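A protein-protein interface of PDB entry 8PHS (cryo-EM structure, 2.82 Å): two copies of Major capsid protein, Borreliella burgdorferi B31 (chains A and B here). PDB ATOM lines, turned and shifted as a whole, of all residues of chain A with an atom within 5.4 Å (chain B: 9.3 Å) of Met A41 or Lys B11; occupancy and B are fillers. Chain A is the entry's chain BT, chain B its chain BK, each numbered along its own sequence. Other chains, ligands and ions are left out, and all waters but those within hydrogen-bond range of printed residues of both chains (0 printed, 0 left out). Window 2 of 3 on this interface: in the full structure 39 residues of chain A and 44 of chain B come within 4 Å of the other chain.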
ATOM      1  N   ASP A  38     -18.736 -26.956  13.102  1.00  0.00           N
ATOM      2  CA  ASP A  38     -19.179 -27.726  14.264  1.00  0.00           C
ATOM      3  C   ASP A  38     -18.512 -27.149  15.506  1.00  0.00           C
ATOM      4  O   ASP A  38     -17.403 -27.533  15.880  1.00  0.00           O
ATOM      5  CB  ASP A  38     -18.856 -29.204  14.086  1.00  0.00           C
ATOM      6  CG  ASP A  38     -19.558 -30.081  15.103  1.00  0.00           C
ATOM      7  OD1 ASP A  38     -20.308 -29.541  15.941  1.00  0.00           O
ATOM      8  OD2 ASP A  38     -19.361 -31.313  15.063  1.00  0.00           O
ATOM      9  N   LEU A  39     -19.203 -26.218  16.158  1.00  0.00           N
ATOM     10  CA  LEU A  39     -18.662 -25.530  17.320  1.00  0.00           C
ATOM     11  C   LEU A  39     -19.807 -24.897  18.098  1.00  0.00           C
ATOM     12  O   LEU A  39     -20.833 -24.532  17.523  1.00  0.00           O
ATOM     13  CB  LEU A  39     -17.639 -24.468  16.899  1.00  0.00           C
ATOM     14  CG  LEU A  39     -16.999 -23.601  17.980  1.00  0.00           C
ATOM     15  CD1 LEU A  39     -16.246 -24.464  18.966  1.00  0.00           C
ATOM     16  CD2 LEU A  39     -16.074 -22.580  17.353  1.00  0.00           C
ATOM     17  N   GLN A  40     -19.623 -24.785  19.412  1.00  0.00           N
ATOM     18  CA  GLN A  40     -20.560 -24.061  20.264  1.00  0.00           C
ATOM     19  C   GLN A  40     -19.943 -22.817  20.881  1.00  0.00           C
ATOM     20  O   GLN A  40     -20.482 -21.719  20.714  1.00  0.00           O
ATOM     21  CB  GLN A  40     -21.104 -24.977  21.370  1.00  0.00           C
ATOM     22  CG  GLN A  40     -22.372 -25.719  20.982  1.00  0.00           C
ATOM     23  CD  GLN A  40     -22.957 -26.513  22.129  1.00  0.00           C
ATOM     24  OE1 GLN A  40     -22.393 -26.557  23.221  1.00  0.00           O
ATOM     25  NE2 GLN A  40     -24.101 -27.144  21.888  1.00  0.00           N
ATOM     26  N   MET A  41     -18.828 -22.955  21.589  1.00  0.00           N
ATOM     27  CA  MET A  41     -18.155 -21.815  22.191  1.00  0.00           C
ATOM     28  C   MET A  41     -16.651 -22.016  22.088  1.00  0.00           C
ATOM     29  O   MET A  41     -16.145 -23.112  22.338  1.00  0.00           O
ATOM     30  CB  MET A  41     -18.567 -21.627  23.656  1.00  0.00           C
ATOM     31  CG  MET A  41     -17.632 -20.735  24.455  1.00  0.00           C
ATOM     32  SD  MET A  41     -18.242 -20.377  26.110  1.00  0.00           S
ATOM     33  CE  MET A  41     -17.587 -18.731  26.357  1.00  0.00           C
ATOM     34  N   GLY A  42     -15.948 -20.952  21.719  1.00  0.00           N
ATOM     35  CA  GLY A  42     -14.518 -21.019  21.510  1.00  0.00           C
ATOM     36  C   GLY A  42     -14.104 -20.184  20.320  1.00  0.00           C
ATOM     37  O   GLY A  42     -14.577 -19.055  20.158  1.00  0.00           O
ATOM     38  N   TYR A  43     -13.228 -20.721  19.477  1.00  0.00           N
ATOM     39  CA  TYR A  43     -12.822 -20.020  18.270  1.00  0.00           C
ATOM     40  C   TYR A  43     -12.352 -21.036  17.240  1.00  0.00           C
ATOM     41  O   TYR A  43     -12.087 -22.199  17.554  1.00  0.00           O
ATOM     42  CB  TYR A  43     -11.752 -18.960  18.575  1.00  0.00           C
ATOM     43  CG  TYR A  43     -10.356 -19.480  18.838  1.00  0.00           C
ATOM     44  CD1 TYR A  43      -9.523 -19.870  17.798  1.00  0.00           C
ATOM     45  CD2 TYR A  43      -9.868 -19.567  20.132  1.00  0.00           C
ATOM     46  CE1 TYR A  43      -8.251 -20.337  18.039  1.00  0.00           C
ATOM     47  CE2 TYR A  43      -8.597 -20.031  20.382  1.00  0.00           C
ATOM     48  CZ  TYR A  43      -7.792 -20.417  19.333  1.00  0.00           C
ATOM     49  OH  TYR A  43      -6.522 -20.883  19.581  1.00  0.00           O
ATOM     50  N   GLN A  44     -12.254 -20.577  15.995  1.00  0.00           N
ATOM     51  CA  GLN A  44     -11.876 -21.418  14.868  1.00  0.00           C
ATOM     52  C   GLN A  44     -10.753 -20.737  14.104  1.00  0.00           C
ATOM     53  O   GLN A  44     -10.924 -19.614  13.618  1.00  0.00           O
ATOM     54  CB  GLN A  44     -13.074 -21.670  13.951  1.00  0.00           C
ATOM     55  CG  GLN A  44     -12.717 -22.229  12.590  1.00  0.00           C
ATOM     56  CD  GLN A  44     -13.839 -22.067  11.590  1.00  0.00           C
ATOM     57  OE1 GLN A  44     -14.882 -21.493  11.900  1.00  0.00           O
ATOM     58  NE2 GLN A  44     -13.631 -22.570  10.380  1.00  0.00           N
ATOM     59  N   TYR A  81     -16.541 -17.434  18.640  1.00  0.00           N
ATOM     60  CA  TYR A  81     -17.939 -17.824  18.732  1.00  0.00           C
ATOM     61  C   TYR A  81     -18.370 -17.800  20.191  1.00  0.00           C
ATOM     62  O   TYR A  81     -17.599 -18.177  21.078  1.00  0.00           O
ATOM     63  CB  TYR A  81     -18.186 -19.219  18.140  1.00  0.00           C
ATOM     64  CG  TYR A  81     -17.910 -19.338  16.656  1.00  0.00           C
ATOM     65  CD1 TYR A  81     -16.615 -19.311  16.161  1.00  0.00           C
ATOM     66  CD2 TYR A  81     -18.951 -19.483  15.752  1.00  0.00           C
ATOM     67  CE1 TYR A  81     -16.366 -19.422  14.808  1.00  0.00           C
ATOM     68  CE2 TYR A  81     -18.713 -19.594  14.400  1.00  0.00           C
ATOM     69  CZ  TYR A  81     -17.419 -19.564  13.932  1.00  0.00           C
ATOM     70  OH  TYR A  81     -17.178 -19.675  12.584  1.00  0.00           O
ATOM     71  N   LEU A  82     -19.600 -17.356  20.436  1.00  0.00           N
ATOM     72  CA  LEU A  82     -20.111 -17.203  21.791  1.00  0.00           C
ATOM     73  C   LEU A  82     -21.463 -17.886  21.925  1.00  0.00           C
ATOM     74  O   LEU A  82     -22.285 -17.840  21.006  1.00  0.00           O
ATOM     75  CB  LEU A  82     -20.227 -15.725  22.166  1.00  0.00           C
ATOM     76  CG  LEU A  82     -20.194 -15.395  23.656  1.00  0.00           C
ATOM     77  CD1 LEU A  82     -18.822 -15.689  24.230  1.00  0.00           C
ATOM     78  CD2 LEU A  82     -20.560 -13.939  23.873  1.00  0.00           C
ATOM     79  N   LYS A  83     -21.694 -18.513  23.075  1.00  0.00           N
ATOM     80  CA  LYS A  83     -22.930 -19.236  23.350  1.00  0.00           C
ATOM     81  C   LYS A  83     -23.814 -18.416  24.281  1.00  0.00           C
ATOM     82  O   LYS A  83     -23.351 -17.933  25.317  1.00  0.00           O
ATOM     83  CB  LYS A  83     -22.630 -20.598  23.976  1.00  0.00           C
ATOM     84  CG  LYS A  83     -23.849 -21.480  24.166  1.00  0.00           C
ATOM     85  CD  LYS A  83     -23.490 -22.737  24.937  1.00  0.00           C
ATOM     86  CE  LYS A  83     -24.686 -23.656  25.089  1.00  0.00           C
ATOM     87  NZ  LYS A  83     -24.341 -24.869  25.879  1.00  0.00           N
ATOM     88  N   ASP B   5      -4.349 -21.383  28.157  1.00  0.00           N
ATOM     89  CA  ASP B   5      -4.309 -22.361  27.069  1.00  0.00           C
ATOM     90  C   ASP B   5      -5.397 -22.013  26.057  1.00  0.00           C
ATOM     91  O   ASP B   5      -6.506 -22.551  26.068  1.00  0.00           O
ATOM     92  CB  ASP B   5      -4.477 -23.777  27.612  1.00  0.00           C
ATOM     93  CG  ASP B   5      -4.259 -24.841  26.549  1.00  0.00           C
ATOM     94  OD1 ASP B   5      -3.906 -24.487  25.407  1.00  0.00           O
ATOM     95  OD2 ASP B   5      -4.449 -26.036  26.857  1.00  0.00           O
ATOM     96  N   GLU B   6      -5.064 -21.086  25.157  1.00  0.00           N
ATOM     97  CA  GLU B   6      -6.014 -20.692  24.125  1.00  0.00           C
ATOM     98  C   GLU B   6      -6.156 -21.749  23.039  1.00  0.00           C
ATOM     99  O   GLU B   6      -7.187 -21.784  22.361  1.00  0.00           O
ATOM    100  CB  GLU B   6      -5.601 -19.357  23.504  1.00  0.00           C
ATOM    101  CG  GLU B   6      -4.287 -19.394  22.747  1.00  0.00           C
ATOM    102  CD  GLU B   6      -3.907 -18.038  22.190  1.00  0.00           C
ATOM    103  OE1 GLU B   6      -4.676 -17.076  22.402  1.00  0.00           O
ATOM    104  OE2 GLU B   6      -2.844 -17.932  21.542  1.00  0.00           O
ATOM    105  N   ASN B   7      -5.154 -22.613  22.866  1.00  0.00           N
ATOM    106  CA  ASN B   7      -5.258 -23.690  21.887  1.00  0.00           C
ATOM    107  C   ASN B   7      -6.382 -24.659  22.223  1.00  0.00           C
ATOM    108  O   ASN B   7      -6.857 -25.375  21.334  1.00  0.00           O
ATOM    109  CB  ASN B   7      -3.932 -24.441  21.791  1.00  0.00           C
ATOM    110  CG  ASN B   7      -2.763 -23.521  21.505  1.00  0.00           C
ATOM    111  OD1 ASN B   7      -2.946 -22.352  21.166  1.00  0.00           O
ATOM    112  ND2 ASN B   7      -1.551 -24.042  21.652  1.00  0.00           N
ATOM    113  N   TYR B   8      -6.813 -24.700  23.486  1.00  0.00           N
ATOM    114  CA  TYR B   8      -7.933 -25.553  23.865  1.00  0.00           C
ATOM    115  C   TYR B   8      -9.219 -25.132  23.167  1.00  0.00           C
ATOM    116  O   TYR B   8     -10.045 -25.983  22.819  1.00  0.00           O
ATOM    117  CB  TYR B   8      -8.118 -25.524  25.382  1.00  0.00           C
ATOM    118  CG  TYR B   8      -9.386 -26.193  25.856  1.00  0.00           C
ATOM    119  CD1 TYR B   8      -9.550 -27.565  25.747  1.00  0.00           C
ATOM    120  CD2 TYR B   8     -10.422 -25.450  26.406  1.00  0.00           C
ATOM    121  CE1 TYR B   8     -10.705 -28.181  26.178  1.00  0.00           C
ATOM    122  CE2 TYR B   8     -11.583 -26.058  26.838  1.00  0.00           C
ATOM    123  CZ  TYR B   8     -11.718 -27.424  26.721  1.00  0.00           C
ATOM    124  OH  TYR B   8     -12.871 -28.037  27.150  1.00  0.00           O
ATOM    125  N   TYR B   9      -9.405 -23.829  22.952  1.00  0.00           N
ATOM    126  CA  TYR B   9     -10.623 -23.317  22.340  1.00  0.00           C
ATOM    127  C   TYR B   9     -10.608 -23.395  20.819  1.00  0.00           C
ATOM    128  O   TYR B   9     -11.643 -23.137  20.196  1.00  0.00           O
ATOM    129  CB  TYR B   9     -10.857 -21.872  22.783  1.00  0.00           C
ATOM    130  CG  TYR B   9     -10.996 -21.724  24.279  1.00  0.00           C
ATOM    131  CD1 TYR B   9     -12.062 -22.300  24.956  1.00  0.00           C
ATOM    132  CD2 TYR B   9     -10.055 -21.020  25.017  1.00  0.00           C
ATOM    133  CE1 TYR B   9     -12.193 -22.172  26.324  1.00  0.00           C
ATOM    134  CE2 TYR B   9     -10.176 -20.887  26.386  1.00  0.00           C
ATOM    135  CZ  TYR B   9     -11.247 -21.466  27.034  1.00  0.00           C
ATOM    136  OH  TYR B   9     -11.373 -21.336  28.397  1.00  0.00           O
ATOM    137  N   ALA B  10      -9.474 -23.741  20.209  1.00  0.00           N
ATOM    138  CA  ALA B  10      -9.397 -23.929  18.760  1.00  0.00           C
ATOM    139  C   ALA B  10     -10.018 -25.281  18.426  1.00  0.00           C
ATOM    140  O   ALA B  10      -9.339 -26.287  18.209  1.00  0.00           O
ATOM    141  CB  ALA B  10      -7.956 -23.834  18.277  1.00  0.00           C
ATOM    142  N   LYS B  11     -11.349 -25.296  18.383  1.00  0.00           N
ATOM    143  CA  LYS B  11     -12.114 -26.521  18.208  1.00  0.00           C
ATOM    144  C   LYS B  11     -12.552 -26.744  16.767  1.00  0.00           C
ATOM    145  O   LYS B  11     -13.326 -27.668  16.501  1.00  0.00           O
ATOM    146  CB  LYS B  11     -13.330 -26.508  19.134  1.00  0.00           C
ATOM    147  CG  LYS B  11     -12.976 -26.304  20.598  1.00  0.00           C
ATOM    148  CD  LYS B  11     -14.213 -26.139  21.459  1.00  0.00           C
ATOM    149  CE  LYS B  11     -13.840 -25.903  22.911  1.00  0.00           C
ATOM    150  NZ  LYS B  11     -13.106 -27.062  23.485  1.00  0.00           N
ATOM    151  N   ALA B  12     -12.077 -25.923  15.835  1.00  0.00           N
ATOM    152  CA  ALA B  12     -12.388 -26.099  14.424  1.00  0.00           C
ATOM    153  C   ALA B  12     -11.270 -25.479  13.602  1.00  0.00           C
ATOM    154  O   ALA B  12     -10.795 -24.386  13.918  1.00  0.00           O
ATOM    155  CB  ALA B  12     -13.736 -25.465  14.062  1.00  0.00           C
ATOM    156  N   VAL B  13     -10.847 -26.186  12.557  1.00  0.00           N
ATOM    157  CA  VAL B  13      -9.791 -25.722  11.666  1.00  0.00           C
ATOM    158  C   VAL B  13     -10.287 -25.830  10.232  1.00  0.00           C
ATOM    159  O   VAL B  13     -10.734 -26.900   9.804  1.00  0.00           O
ATOM    160  CB  VAL B  13      -8.488 -26.524  11.850  1.00  0.00           C
ATOM    161  CG1 VAL B  13      -7.467 -26.117  10.803  1.00  0.00           C
ATOM    162  CG2 VAL B  13      -7.930 -26.314  13.247  1.00  0.00           C
ATOM    163  N   ALA B  14     -10.207 -24.726   9.495  1.00  0.00           N
ATOM    164  CA  ALA B  14     -10.563 -24.684   8.084  1.00  0.00           C
ATOM    165  C   ALA B  14      -9.363 -24.191   7.294  1.00  0.00           C
ATOM    166  O   ALA B  14      -8.750 -23.181   7.656  1.00  0.00           O
ATOM    167  CB  ALA B  14     -11.773 -23.778   7.841  1.00  0.00           C
ATOM    168  N   SER B 103      -5.408 -31.181  12.273  1.00  0.00           N
ATOM    169  CA  SER B 103      -5.638 -29.744  12.255  1.00  0.00           C
ATOM    170  C   SER B 103      -4.583 -28.992  11.457  1.00  0.00           C
ATOM    171  O   SER B 103      -4.547 -27.759  11.504  1.00  0.00           O
ATOM    172  CB  SER B 103      -5.695 -29.205  13.686  1.00  0.00           C
ATOM    173  OG  SER B 103      -4.513 -29.527  14.398  1.00  0.00           O
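No position is printed for both chains.
Of the 10 pairs that touch across the chains among the printed residues, none has its exchanged pair printed and touching as well.
Gln A40 touches none of the printed residues of chain B.
Met A41 touches one residue of chain B.
Printed residues of chain B within 4 Å of Gln A44: Ala B12 (3.2 Å) and Ala B14 (3.4 Å).
Tyr A81 touches none of the printed residues of chain B.
Of the printed residues of chain A, Glu B6 touches Tyr A43 (3.0 Å).
Of the printed residues of chain A, Tyr B9 touches Gly A42 and Tyr A43.
Of the printed residues of chain A, Ala B12 touches Gln A44.
The nearest printed residue of chain A that does not touch Ala B12 is Tyr A43 (4.1 Å).
Among the printed residues, pairs that only touch across the chains: Leu A39 with Lys B11, Met A41 with Lys B11, Gly A42 with Tyr B9, Tyr A43 with Asn B7, Tyr A43 with Ala B10, Gln A44 with Ala B12 and Gln A44 with Ala B14.
Of the 10 printed residues of chain A, 5 touch a printed residue of chain B.
Printed residues of chain A that touch a printed residue of chain B: Leu A39, Met A41, Gly A42, Tyr A43 and Gln A44.
Hydrophobic or aromatic side chains of chain A that line the printed part of chain B: Leu A39 and Tyr A43.
Hydrophobic or aromatic side chains of chain B within 4 Å of the printed part of chain A: Tyr B9, Ala B10, Ala B12 and Ala B14.
Along chain B the printed residues that touch a printed residue of chain A span positions 6 to 14.
Among the printed residues, no Asp or Glu carboxylate lies within 4 Å of a Lys or Arg side-chain nitrogen of the other chain.
The backbone NH (N) of Tyr A81 sits at hydrogen-bond distance from the backbone carbonyl oxygen (O) of Gly A42.
OE1 of Gln A44 lies within hydrogen-bond range of OH of Tyr A81, 3.0 Å away.
The backbone NH (N) of Asn B7 sits close to the side-chain carboxylate (OD1) of Asp B5 (3.4 Å).
NZ of Lys B11 lies within hydrogen-bond range of O of Tyr B8, at 3.3 Å.
The backbone NH (N) of Lys B11 sits at hydrogen-bond distance from the backbone carbonyl oxygen (O) of Tyr A43 (3.3 Å).
The backbone carbonyl oxygen of Glu B6 lies close to the side-chain hydroxyl of Tyr A43, 3.0 Å away.
The backbone NH of Tyr A43 sits at hydrogen-bond distance from the backbone carbonyl oxygen of Tyr B9, at 3.0 Å.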
